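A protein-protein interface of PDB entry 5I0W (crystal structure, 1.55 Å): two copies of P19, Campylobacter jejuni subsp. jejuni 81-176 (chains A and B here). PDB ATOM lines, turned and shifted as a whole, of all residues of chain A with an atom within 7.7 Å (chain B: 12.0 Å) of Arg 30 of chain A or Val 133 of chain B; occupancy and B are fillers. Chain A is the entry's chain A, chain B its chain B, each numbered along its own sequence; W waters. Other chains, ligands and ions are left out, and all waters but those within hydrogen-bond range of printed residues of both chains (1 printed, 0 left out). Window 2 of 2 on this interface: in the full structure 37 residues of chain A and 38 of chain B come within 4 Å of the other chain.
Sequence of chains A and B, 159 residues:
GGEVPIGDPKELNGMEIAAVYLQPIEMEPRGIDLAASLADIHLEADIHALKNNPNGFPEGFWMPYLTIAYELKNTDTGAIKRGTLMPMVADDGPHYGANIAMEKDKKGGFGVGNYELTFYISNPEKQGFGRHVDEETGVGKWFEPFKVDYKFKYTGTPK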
ATOM      1  N   ILE A  25      19.317   1.483 -24.181  1.00  0.00           N
ATOM      2  CA  ILE A  25      20.081   0.263 -23.919  1.00  0.00           C
ATOM      3  C   ILE A  25      21.582   0.528 -23.920  1.00  0.00           C
ATOM      4  O   ILE A  25      22.080   1.369 -24.673  1.00  0.00           O
ATOM      5  CB  ILE A  25      19.760  -0.835 -24.946  1.00  0.00           C
ATOM      6  CG1 ILE A  25      20.198  -0.387 -26.335  1.00  0.00           C
ATOM      7  CG2 ILE A  25      18.279  -1.177 -24.934  1.00  0.00           C
ATOM      8  CD1 ILE A  25      21.696  -0.360 -26.533  1.00  0.00           C
ATOM      9  N   GLU A  26      22.300  -0.204 -23.074  1.00  0.00           N
ATOM     10  CA  GLU A  26      23.743  -0.027 -22.935  1.00  0.00           C
ATOM     11  C   GLU A  26      24.344  -0.892 -24.016  1.00  0.00           C
ATOM     12  O   GLU A  26      24.009  -2.076 -24.095  1.00  0.00           O
ATOM     13  CB  GLU A  26      24.228  -0.534 -21.586  1.00  0.00           C
ATOM     14  CG  GLU A  26      23.495   0.027 -20.383  1.00  0.00           C
ATOM     15  CD  GLU A  26      24.049   1.353 -19.913  1.00  0.00           C
ATOM     16  OE1 GLU A  26      25.090   1.788 -20.444  1.00  0.00           O
ATOM     17  OE2 GLU A  26      23.441   1.958 -19.004  1.00  0.00           O
ATOM     18  N   MET A  27      25.217  -0.312 -24.839  1.00  0.00           N
ATOM     19  CA  MET A  27      25.782  -1.027 -25.990  1.00  0.00           C
ATOM     20  C   MET A  27      27.300  -1.035 -25.931  1.00  0.00           C
ATOM     21  O   MET A  27      27.919  -0.056 -25.493  1.00  0.00           O
ATOM     22  CB  MET A  27      25.337  -0.388 -27.316  1.00  0.00           C
ATOM     23  CG  MET A  27      25.420  -1.315 -28.535  1.00  0.00           C
ATOM     24  SD  MET A  27      25.487  -0.462 -30.130  1.00  0.00           S
ATOM     25  CE  MET A  27      27.101   0.309 -30.020  1.00  0.00           C
ATOM     26  N   GLU A  28      27.898  -2.153 -26.339  1.00  0.00           N
ATOM     27  CA  GLU A  28      29.336  -2.224 -26.587  1.00  0.00           C
ATOM     28  C   GLU A  28      29.521  -2.330 -28.109  1.00  0.00           C
ATOM     29  O   GLU A  28      28.604  -2.783 -28.797  1.00  0.00           O
ATOM     30  CB  GLU A  28      29.962  -3.420 -25.859  1.00  0.00           C
ATOM     31  CG  GLU A  28      30.037  -3.272 -24.344  1.00  0.00           C
ATOM     32  CD  GLU A  28      31.138  -2.334 -23.876  1.00  0.00           C
ATOM     33  OE1 GLU A  28      31.154  -1.986 -22.673  1.00  0.00           O
ATOM     34  OE2 GLU A  28      31.990  -1.942 -24.700  1.00  0.00           O
ATOM     35  N   PRO A  29      30.664  -1.857 -28.653  1.00  0.00           N
ATOM     36  CA  PRO A  29      31.727  -1.128 -27.950  1.00  0.00           C
ATOM     37  C   PRO A  29      31.260   0.254 -27.482  1.00  0.00           C
ATOM     38  O   PRO A  29      30.438   0.894 -28.146  1.00  0.00           O
ATOM     39  CB  PRO A  29      32.822  -0.988 -29.011  1.00  0.00           C
ATOM     40  CG  PRO A  29      32.101  -1.011 -30.311  1.00  0.00           C
ATOM     41  CD  PRO A  29      30.941  -1.951 -30.102  1.00  0.00           C
ATOM     42  N   ARG A  30      31.787   0.690 -26.341  1.00  0.00           N
ATOM     43  CA  ARG A  30      31.469   1.994 -25.767  1.00  0.00           C
ATOM     44  C   ARG A  30      31.955   3.098 -26.686  1.00  0.00           C
ATOM     45  O   ARG A  30      33.021   2.971 -27.291  1.00  0.00           O
ATOM     46  CB  ARG A  30      32.169   2.138 -24.415  1.00  0.00           C
ATOM     47  CG  ARG A  30      32.051   0.926 -23.505  1.00  0.00           C
ATOM     48  CD  ARG A  30      31.161   1.221 -22.310  1.00  0.00           C
ATOM     49  NE  ARG A  30      29.739   1.109 -22.614  1.00  0.00           N
ATOM     50  CZ  ARG A  30      28.953   0.155 -22.128  1.00  0.00           C
ATOM     51  NH1 ARG A  30      29.460  -0.766 -21.320  1.00  0.00           N
ATOM     52  NH2 ARG A  30      27.668   0.126 -22.442  1.00  0.00           N
ATOM     53  N   GLY A  31      31.171   4.168 -26.797  1.00  0.00           N
ATOM     54  CA  GLY A  31      31.567   5.347 -27.549  1.00  0.00           C
ATOM     55  C   GLY A  31      31.044   5.465 -28.962  1.00  0.00           C
ATOM     56  O   GLY A  31      31.129   6.539 -29.552  1.00  0.00           O
ATOM     57  N   ILE A  32      30.473   4.391 -29.505  1.00  0.00           N
ATOM     58  CA  ILE A  32      29.976   4.429 -30.888  1.00  0.00           C
ATOM     59  C   ILE A  32      28.478   4.727 -31.031  1.00  0.00           C
ATOM     60  O   ILE A  32      28.016   5.029 -32.131  1.00  0.00           O
ATOM     61  CB  ILE A  32      30.378   3.175 -31.697  1.00  0.00           C
ATOM     62  CG1 ILE A  32      30.235   3.440 -33.199  1.00  0.00           C
ATOM     63  CG2 ILE A  32      29.595   1.955 -31.242  1.00  0.00           C
ATOM     64  CD1 ILE A  32      28.978   4.193 -33.577  1.00  0.00           C
ATOM     65  N   ASP A  33      27.731   4.635 -29.928  1.00  0.00           N
ATOM     66  CA  ASP A  33      26.398   5.211 -29.849  1.00  0.00           C
ATOM     67  C   ASP A  33      26.203   6.051 -28.600  1.00  0.00           C
ATOM     68  O   ASP A  33      26.992   5.970 -27.647  1.00  0.00           O
ATOM     69  CB  ASP A  33      25.311   4.151 -29.935  1.00  0.00           C
ATOM     70  CG  ASP A  33      23.990   4.733 -30.412  1.00  0.00           C
ATOM     71  OD1 ASP A  33      24.005   5.772 -31.104  1.00  0.00           O
ATOM     72  OD2 ASP A  33      22.946   4.171 -30.088  1.00  0.00           O
ATOM     73  N   ALA A  35      25.275   7.314 -25.157  1.00  0.00           N
ATOM     74  CA  ALA A  35      25.173   6.664 -23.851  1.00  0.00           C
ATOM     75  C   ALA A  35      23.725   6.540 -23.369  1.00  0.00           C
ATOM     76  O   ALA A  35      22.906   7.448 -23.577  1.00  0.00           O
ATOM     77  CB  ALA A  35      26.012   7.417 -22.828  1.00  0.00           C
ATOM     78  N   ALA A  36      23.402   5.411 -22.739  1.00  0.00           N
ATOM     79  CA  ALA A  36      22.042   5.178 -22.237  1.00  0.00           C
ATOM     80  C   ALA A  36      21.552   6.281 -21.294  1.00  0.00           C
ATOM     81  O   ALA A  36      20.394   6.709 -21.363  1.00  0.00           O
ATOM     82  CB  ALA A  36      21.950   3.819 -21.556  1.00  0.00           C
ATOM     83  N   VAL A  89      23.381  -6.642 -32.064  1.00  0.00           N
ATOM     84  CA  VAL A  89      22.621  -7.777 -31.616  1.00  0.00           C
ATOM     85  C   VAL A  89      22.157  -7.632 -30.160  1.00  0.00           C
ATOM     86  O   VAL A  89      22.898  -7.090 -29.307  1.00  0.00           O
ATOM     87  CB  VAL A  89      23.422  -9.085 -31.898  1.00  0.00           C
ATOM     88  CG1 VAL A  89      24.648  -9.208 -30.974  1.00  0.00           C
ATOM     89  CG2 VAL A  89      22.489 -10.286 -31.791  1.00  0.00           C
ATOM     90  N   ALA A  90      20.934  -8.097 -29.899  1.00  0.00           N
ATOM     91  CA  ALA A  90      20.362  -8.207 -28.554  1.00  0.00           C
ATOM     92  C   ALA A  90      20.021  -9.671 -28.302  1.00  0.00           C
ATOM     93  O   ALA A  90      20.252 -10.539 -29.165  1.00  0.00           O
ATOM     94  CB  ALA A  90      19.121  -7.319 -28.429  1.00  0.00           C
ATOM     95  N   PRO B  54      25.577 -17.631 -27.787  1.00  0.00           N
ATOM     96  CA  PRO B  54      25.771 -16.752 -26.627  1.00  0.00           C
ATOM     97  C   PRO B  54      25.753 -15.262 -26.944  1.00  0.00           C
ATOM     98  O   PRO B  54      25.747 -14.412 -26.031  1.00  0.00           O
ATOM     99  CB  PRO B  54      27.159 -17.174 -26.120  1.00  0.00           C
ATOM    100  CG  PRO B  54      27.884 -17.557 -27.377  1.00  0.00           C
ATOM    101  CD  PRO B  54      26.826 -18.281 -28.212  1.00  0.00           C
ATOM    102  N   ASN B  55      25.722 -14.935 -28.235  1.00  0.00           N
ATOM    103  CA  ASN B  55      25.716 -13.545 -28.662  1.00  0.00           C
ATOM    104  C   ASN B  55      24.348 -13.155 -29.211  1.00  0.00           C
ATOM    105  O   ASN B  55      24.213 -12.132 -29.844  1.00  0.00           O
ATOM    106  CB  ASN B  55      26.839 -13.322 -29.671  1.00  0.00           C
ATOM    107  CG  ASN B  55      28.180 -13.744 -29.112  1.00  0.00           C
ATOM    108  OD1 ASN B  55      28.783 -14.719 -29.568  1.00  0.00           O
ATOM    109  ND2 ASN B  55      28.630 -13.038 -28.089  1.00  0.00           N
ATOM    110  N   GLY B  56      23.333 -13.981 -28.946  1.00  0.00           N
ATOM    111  CA  GLY B  56      21.932 -13.620 -29.246  1.00  0.00           C
ATOM    112  C   GLY B  56      21.450 -13.965 -30.647  1.00  0.00           C
ATOM    113  O   GLY B  56      20.332 -13.605 -31.027  1.00  0.00           O
ATOM    114  N   ASN B 123      35.690 -11.356 -34.766  1.00  0.00           N
ATOM    115  CA  ASN B 123      34.300 -11.089 -34.429  1.00  0.00           C
ATOM    116  C   ASN B 123      33.720  -9.809 -35.062  1.00  0.00           C
ATOM    117  O   ASN B 123      34.470  -8.976 -35.582  1.00  0.00           O
ATOM    118  CB  ASN B 123      34.118 -11.134 -32.904  1.00  0.00           C
ATOM    119  CG  ASN B 123      34.688  -9.912 -32.196  1.00  0.00           C
ATOM    120  OD1 ASN B 123      34.467  -8.779 -32.610  1.00  0.00           O
ATOM    121  ND2 ASN B 123      35.418 -10.147 -31.096  1.00  0.00           N
ATOM    122  N   PRO B 124      32.389  -9.664 -35.053  1.00  0.00           N
ATOM    123  CA  PRO B 124      31.720  -8.559 -35.726  1.00  0.00           C
ATOM    124  C   PRO B 124      32.096  -7.170 -35.223  1.00  0.00           C
ATOM    125  O   PRO B 124      31.971  -6.199 -35.976  1.00  0.00           O
ATOM    126  CB  PRO B 124      30.233  -8.850 -35.461  1.00  0.00           C
ATOM    127  CG  PRO B 124      30.206 -10.347 -35.438  1.00  0.00           C
ATOM    128  CD  PRO B 124      31.420 -10.694 -34.627  1.00  0.00           C
ATOM    129  N   GLU B 125      32.536  -7.069 -33.974  1.00  0.00           N
ATOM    130  CA  GLU B 125      32.903  -5.766 -33.431  1.00  0.00           C
ATOM    131  C   GLU B 125      34.041  -5.119 -34.227  1.00  0.00           C
ATOM    132  O   GLU B 125      34.119  -3.894 -34.304  1.00  0.00           O
ATOM    133  CB  GLU B 125      33.263  -5.853 -31.941  1.00  0.00           C
ATOM    134  CG  GLU B 125      33.273  -4.497 -31.257  1.00  0.00           C
ATOM    135  CD  GLU B 125      33.211  -4.602 -29.752  1.00  0.00           C
ATOM    136  OE1 GLU B 125      34.214  -4.260 -29.093  1.00  0.00           O
ATOM    137  OE2 GLU B 125      32.163  -5.036 -29.223  1.00  0.00           O
ATOM    138  N   LYS B 126      34.911  -5.942 -34.823  1.00  0.00           N
ATOM    139  CA  LYS B 126      36.040  -5.442 -35.610  1.00  0.00           C
ATOM    140  C   LYS B 126      35.535  -4.556 -36.731  1.00  0.00           C
ATOM    141  O   LYS B 126      36.242  -3.653 -37.176  1.00  0.00           O
ATOM    142  CB  LYS B 126      36.865  -6.604 -36.184  1.00  0.00           C
ATOM    143  CG  LYS B 126      38.152  -6.183 -36.870  1.00  0.00           C
ATOM    144  CD  LYS B 126      38.832  -7.375 -37.513  1.00  0.00           C
ATOM    145  CE  LYS B 126      40.046  -6.964 -38.329  1.00  0.00           C
ATOM    146  NZ  LYS B 126      41.144  -6.506 -37.431  1.00  0.00           N
ATOM    147  N   GLN B 127      34.300  -4.814 -37.163  1.00  0.00           N
ATOM    148  CA  GLN B 127      33.634  -4.011 -38.182  1.00  0.00           C
ATOM    149  C   GLN B 127      32.591  -3.035 -37.615  1.00  0.00           C
ATOM    150  O   GLN B 127      31.813  -2.464 -38.362  1.00  0.00           O
ATOM    151  CB  GLN B 127      33.021  -4.915 -39.253  1.00  0.00           C
ATOM    152  CG  GLN B 127      34.059  -5.619 -40.108  1.00  0.00           C
ATOM    153  CD  GLN B 127      33.451  -6.547 -41.143  1.00  0.00           C
ATOM    154  OE1 GLN B 127      32.341  -6.336 -41.613  1.00  0.00           O
ATOM    155  NE2 GLN B 127      34.187  -7.600 -41.494  1.00  0.00           N
ATOM    156  N   GLY B 128      32.591  -2.845 -36.301  1.00  0.00           N
ATOM    157  CA  GLY B 128      31.694  -1.872 -35.658  1.00  0.00           C
ATOM    158  C   GLY B 128      30.278  -2.329 -35.329  1.00  0.00           C
ATOM    159  O   GLY B 128      29.433  -1.524 -34.932  1.00  0.00           O
ATOM    160  N   PHE B 129      30.002  -3.609 -35.525  1.00  0.00           N
ATOM    161  CA  PHE B 129      28.736  -4.204 -35.128  1.00  0.00           C
ATOM    162  C   PHE B 129      28.648  -4.227 -33.603  1.00  0.00           C
ATOM    163  O   PHE B 129      29.587  -4.653 -32.934  1.00  0.00           O
ATOM    164  CB  PHE B 129      28.696  -5.627 -35.717  1.00  0.00           C
ATOM    165  CG  PHE B 129      27.395  -6.358 -35.517  1.00  0.00           C
ATOM    166  CD1 PHE B 129      27.181  -7.133 -34.391  1.00  0.00           C
ATOM    167  CD2 PHE B 129      26.399  -6.309 -36.489  1.00  0.00           C
ATOM    168  CE1 PHE B 129      25.989  -7.835 -34.222  1.00  0.00           C
ATOM    169  CE2 PHE B 129      25.207  -7.010 -36.332  1.00  0.00           C
ATOM    170  CZ  PHE B 129      24.995  -7.769 -35.193  1.00  0.00           C
ATOM    171  N   GLY B 130      27.523  -3.770 -33.060  1.00  0.00           N
ATOM    172  CA  GLY B 130      27.355  -3.624 -31.607  1.00  0.00           C
ATOM    173  C   GLY B 130      26.648  -4.783 -30.943  1.00  0.00           C
ATOM    174  O   GLY B 130      26.127  -5.684 -31.600  1.00  0.00           O
ATOM    175  N   ARG B 131      26.636  -4.764 -29.615  1.00  0.00           N
ATOM    176  CA  ARG B 131      25.884  -5.742 -28.849  1.00  0.00           C
ATOM    177  C   ARG B 131      25.274  -5.036 -27.651  1.00  0.00           C
ATOM    178  O   ARG B 131      25.946  -4.200 -27.004  1.00  0.00           O
ATOM    179  CB  ARG B 131      26.738  -6.953 -28.421  1.00  0.00           C
ATOM    180  CG  ARG B 131      27.843  -6.666 -27.408  1.00  0.00           C
ATOM    181  CD  ARG B 131      28.704  -7.902 -27.145  1.00  0.00           C
ATOM    182  NE  ARG B 131      29.784  -7.515 -26.239  1.00  0.00           N
ATOM    183  CZ  ARG B 131      29.830  -7.689 -24.919  1.00  0.00           C
ATOM    184  NH1 ARG B 131      28.880  -8.330 -24.231  1.00  0.00           N
ATOM    185  NH2 ARG B 131      30.886  -7.220 -24.277  1.00  0.00           N
ATOM    186  N   HIS B 132      24.028  -5.371 -27.349  1.00  0.00           N
ATOM    187  CA  HIS B 132      23.423  -4.948 -26.076  1.00  0.00           C
ATOM    188  C   HIS B 132      24.130  -5.601 -24.918  1.00  0.00           C
ATOM    189  O   HIS B 132      24.493  -6.791 -24.980  1.00  0.00           O
ATOM    190  CB  HIS B 132      21.945  -5.292 -26.026  1.00  0.00           C
ATOM    191  CG  HIS B 132      21.080  -4.513 -27.003  1.00  0.00           C
ATOM    192  ND1 HIS B 132      19.751  -4.336 -26.795  1.00  0.00           N
ATOM    193  CD2 HIS B 132      21.386  -3.856 -28.199  1.00  0.00           C
ATOM    194  CE1 HIS B 132      19.226  -3.609 -27.831  1.00  0.00           C
ATOM    195  NE2 HIS B 132      20.221  -3.312 -28.676  1.00  0.00           N
ATOM    196  N   VAL B 133      24.332  -4.843 -23.840  1.00  0.00           N
ATOM    197  CA  VAL B 133      24.957  -5.392 -22.621  1.00  0.00           C
ATOM    198  C   VAL B 133      24.158  -5.090 -21.340  1.00  0.00           C
ATOM    199  O   VAL B 133      24.622  -5.372 -20.223  1.00  0.00           O
ATOM    200  CB  VAL B 133      26.450  -4.961 -22.473  1.00  0.00           C
ATOM    201  CG1 VAL B 133      27.252  -5.416 -23.683  1.00  0.00           C
ATOM    202  CG2 VAL B 133      26.607  -3.443 -22.286  1.00  0.00           C
ATOM    203  N   ASP B 134      22.959  -4.548 -21.490  1.00  0.00           N
ATOM    204  CA  ASP B 134      22.133  -4.247 -20.320  1.00  0.00           C
ATOM    205  C   ASP B 134      21.557  -5.544 -19.754  1.00  0.00           C
ATOM    206  O   ASP B 134      21.587  -6.591 -20.411  1.00  0.00           O
ATOM    207  CB  ASP B 134      21.005  -3.313 -20.709  1.00  0.00           C
ATOM    208  CG  ASP B 134      20.386  -3.704 -22.002  1.00  0.00           C
ATOM    209  OD1 ASP B 134      21.007  -3.389 -23.047  1.00  0.00           O
ATOM    210  OD2 ASP B 134      19.318  -4.343 -21.952  1.00  0.00           O
ATOM    211  N   GLU B 135      21.041  -5.482 -18.526  1.00  0.00           N
ATOM    212  CA  GLU B 135      20.512  -6.681 -17.875  1.00  0.00           C
ATOM    213  C   GLU B 135      19.338  -7.302 -18.639  1.00  0.00           C
ATOM    214  O   GLU B 135      19.193  -8.524 -18.701  1.00  0.00           O
ATOM    215  CB  GLU B 135      20.098  -6.384 -16.426  1.00  0.00           C
ATOM    216  CG  GLU B 135      19.846  -7.663 -15.647  1.00  0.00           C
ATOM    217  CD  GLU B 135      19.779  -7.461 -14.153  1.00  0.00           C
ATOM    218  OE1 GLU B 135      20.704  -6.850 -13.569  1.00  0.00           O
ATOM    219  OE2 GLU B 135      18.796  -7.959 -13.566  1.00  0.00           O
ATOM    220  N   GLU B 136      18.531  -6.438 -19.236  1.00  0.00           N
ATOM    221  CA  GLU B 136      17.252  -6.814 -19.801  1.00  0.00           C
ATOM    222  C   GLU B 136      17.404  -7.531 -21.158  1.00  0.00           C
ATOM    223  O   GLU B 136      16.744  -8.542 -21.405  1.00  0.00           O
ATOM    224  CB  GLU B 136      16.386  -5.552 -19.943  1.00  0.00           C
ATOM    225  CG  GLU B 136      15.841  -4.972 -18.625  1.00  0.00           C
ATOM    226  CD  GLU B 136      16.889  -4.334 -17.713  1.00  0.00           C
ATOM    227  OE1 GLU B 136      17.958  -3.891 -18.191  1.00  0.00           O
ATOM    228  OE2 GLU B 136      16.625  -4.265 -16.488  1.00  0.00           O
ATOM    229  N   THR B 137      18.282  -7.018 -22.017  1.00  0.00           N
ATOM    230  CA  THR B 137      18.360  -7.509 -23.403  1.00  0.00           C
ATOM    231  C   THR B 137      19.781  -7.886 -23.832  1.00  0.00           C
ATOM    232  O   THR B 137      20.025  -8.193 -25.016  1.00  0.00           O
ATOM    233  CB  THR B 137      17.816  -6.462 -24.405  1.00  0.00           C
ATOM    234  OG1 THR B 137      18.689  -5.336 -24.463  1.00  0.00           O
ATOM    235  CG2 THR B 137      16.407  -5.983 -23.995  1.00  0.00           C
ATOM    236  N   GLY B 138      20.713  -7.890 -22.880  1.00  0.00           N
ATOM    237  CA  GLY B 138      22.122  -8.012 -23.216  1.00  0.00           C
ATOM    238  C   GLY B 138      22.569  -9.411 -23.575  1.00  0.00           C
ATOM    239  O   GLY B 138      21.884 -10.394 -23.272  1.00  0.00           O
ATOM    240  N   VAL B 139      23.718  -9.488 -24.228  1.00  0.00           N
ATOM    241  CA  VAL B 139      24.319 -10.756 -24.616  1.00  0.00           C
ATOM    242  C   VAL B 139      25.765 -10.793 -24.153  1.00  0.00           C
ATOM    243  O   VAL B 139      26.333  -9.764 -23.743  1.00  0.00           O
ATOM    244  CB  VAL B 139      24.244 -10.984 -26.155  1.00  0.00           C
ATOM    245  CG1 VAL B 139      22.799 -10.889 -26.624  1.00  0.00           C
ATOM    246  CG2 VAL B 139      25.104  -9.975 -26.906  1.00  0.00           C
ATOM    247  N   GLY B 140      26.391 -11.961 -24.241  1.00  0.00           N
ATOM    248  CA  GLY B 140      27.752 -12.103 -23.745  1.00  0.00           C
ATOM    249  C   GLY B 140      28.822 -11.575 -24.699  1.00  0.00           C
ATOM    250  O   GLY B 140      28.530 -11.127 -25.819  1.00  0.00           O
ATOM    251  N   LYS B 141      30.069 -11.662 -24.257  1.00  0.00           N
ATOM    252  CA  LYS B 141      31.212 -11.188 -25.020  1.00  0.00           C
ATOM    253  C   LYS B 141      31.423 -12.023 -26.273  1.00  0.00           C
ATOM    254  O   LYS B 141      31.068 -13.185 -26.321  1.00  0.00           O
ATOM    255  CB  LYS B 141      32.489 -11.330 -24.189  1.00  0.00           C
ATOM    256  CG  LYS B 141      32.702 -10.316 -23.078  1.00  0.00           C
ATOM    257  CD  LYS B 141      34.049 -10.646 -22.439  1.00  0.00           C
ATOM    258  CE  LYS B 141      34.544  -9.541 -21.530  1.00  0.00           C
ATOM    259  NZ  LYS B 141      35.931  -9.865 -21.092  1.00  0.00           N
ATOM    260  N   TRP B 142      32.066 -11.425 -27.259  1.00  0.00           N
ATOM    261  CA  TRP B 142      32.462 -12.099 -28.464  1.00  0.00           C
ATOM    262  C   TRP B 142      33.730 -12.882 -28.293  1.00  0.00           C
ATOM    263  O   TRP B 142      34.641 -12.476 -27.529  1.00  0.00           O
ATOM    264  CB  TRP B 142      32.782 -11.045 -29.502  1.00  0.00           C
ATOM    265  CG  TRP B 142      31.614 -10.231 -29.967  1.00  0.00           C
ATOM    266  CD1 TRP B 142      31.363  -8.889 -29.715  1.00  0.00           C
ATOM    267  CD2 TRP B 142      30.539 -10.675 -30.811  1.00  0.00           C
ATOM    268  NE1 TRP B 142      30.205  -8.484 -30.329  1.00  0.00           N
ATOM    269  CE2 TRP B 142      29.652  -9.514 -30.994  1.00  0.00           C
ATOM    270  CE3 TRP B 142      30.196 -11.886 -31.393  1.00  0.00           C
ATOM    271  CZ2 TRP B 142      28.504  -9.591 -31.763  1.00  0.00           C
ATOM    272  CZ3 TRP B 142      29.029 -11.949 -32.166  1.00  0.00           C
ATOM    273  CH2 TRP B 142      28.209 -10.835 -32.337  1.00  0.00           C
HETATM  274  O   HOH W   1      34.243  -3.125 -26.327  1.00  0.00           O
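The backbone NH (N) of Val 133 of chain B sits at hydrogen-bond distance from the backbone carbonyl oxygen (O) of Glu 26 of chain A, 2.8 Å away.
N of Glu 26 of chain A sits at hydrogen-bond distance from OD1 of Asp 134 of chain B.
O of Val 89 of chain A is in hydrogen-bond range of N of His 132 of chain B.
The backbone NH of Val 89 of chain A lies within hydrogen-bond range of the backbone carbonyl oxygen of Gly 130 of chain B, at 2.9 Å.
The backbone carbonyl oxygen (O) of Arg 131 of chain B sits at hydrogen-bond distance from the backbone NH (N) of Glu 28 of chain A, at 2.9 Å.
NH1 of Arg 131 of chain B sits at hydrogen-bond distance from O of Gly 140 of chain B (3.2 Å).
OG1 of Thr 137 of chain B lies within hydrogen-bond range of ND1 of His 132 of chain B, 2.8 Å away.
OE1 of Glu 28 of chain A is in salt-bridge range of NH1 of Arg 30 of chain A.
The guanidinium group (NH1) of Arg 131 of chain B is in hydrogen-bond range of the backbone carbonyl oxygen (O) of Val 139 of chain B (3.0 Å).
N of Glu 125 of chain B is in hydrogen-bond range of OD1 of Asn 123 of chain B.
O of Pro 124 of chain B sits at hydrogen-bond distance from N of Phe 129 of chain B, 3.3 Å away.
Among the printed residues, pairs that only touch across the chains: Val 89 of chain A with Asn 55 of chain B (3.2 Å), Glu 28 of chain A with Gly 130 of chain B (3.2 Å), Val 89 of chain A with Arg 131 of chain B (3.3 Å), Met 27 of chain A with Arg 131 of chain B (3.3 Å), Ile 25 of chain A with Asp 134 of chain B (3.4 Å), Pro 29 of chain A with Glu 125 of chain B (3.4 Å), Ala 90 of chain A with His 132 of chain B (3.5 Å), Ala 90 of chain A with Val 139 of chain B (3.5 Å), Ala 90 of chain A with Gly 56 of chain B (3.5 Å), Glu 26 of chain A with His 132 of chain B (3.5 Å), Ala 90 of chain A with Thr 137 of chain B (3.6 Å), Glu 28 of chain A with Val 133 of chain B (3.6 Å), Val 89 of chain A with Phe 129 of chain B (3.6 Å), Ile 25 of chain A with His 132 of chain B (3.7 Å), Arg 30 of chain A with Val 133 of chain B (3.7 Å), Glu 28 of chain A with Glu 125 of chain B (3.9 Å), Val 89 of chain A with Trp 142 of chain B (3.95 Å), Met 27 of chain A with Gly 130 of chain B (3.96 Å) and Val 89 of chain A with Gly 56 of chain B (3.99 Å).
Of the printed residues of chain B, Arg 30 of chain A touches Val 133 (3.7 Å).
Of the printed residues of chain B, Glu 26 of chain A touches His 132, Val 133 and Asp 134.
Of chain B, only Gly 130 and Arg 131 come within 4 Å of Met 27 of chain A.
Printed residues of chain A within 4 Å of Phe 129 of chain B: Val 89 (3.6 Å).
Printed residues of chain A within 4 Å of Asn 55 of chain B: Val 89 (3.2 Å).
Gly 140 of chain B touches none of the printed residues of chain A.
Pro 54 of chain B touches none of the printed residues of chain A.
The nearest printed residue of chain B that does not touch Arg 30 of chain A is Glu 125 of chain B (6.2 Å).
The nearest printed residue of chain A that does not touch Val 133 of chain B is Met 27 of chain A (4.3 Å).
The nearest printed residue of chain A that does not touch Gly 56 of chain B is Glu 28 of chain A (12.4 Å).
Printed residues of chain B that touch a printed residue of chain A: Asn 55, Gly 56, Glu 125, Phe 129, Gly 130, Arg 131, His 132, Val 133, Asp 134, Thr 137, Val 139 and Trp 142.
Hydrophobic or aromatic side chains of chain B within 4 Å of the printed part of chain A: Phe 129, His 132, Val 133, Val 139 and Trp 142.
Among the printed residues, no Asp or Glu carboxylate lies within 4 Å of a Lys or Arg side-chain nitrogen of the other chain.
No position is printed for both chains.
Of the 24 pairs that touch across the chains among the printed residues, none has its exchanged pair printed and touching as well.
Water W1 bridges OE1 of Glu 125 of chain B (3.0 Å) and OE2 of Glu 28 of chain A (3.0 Å).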
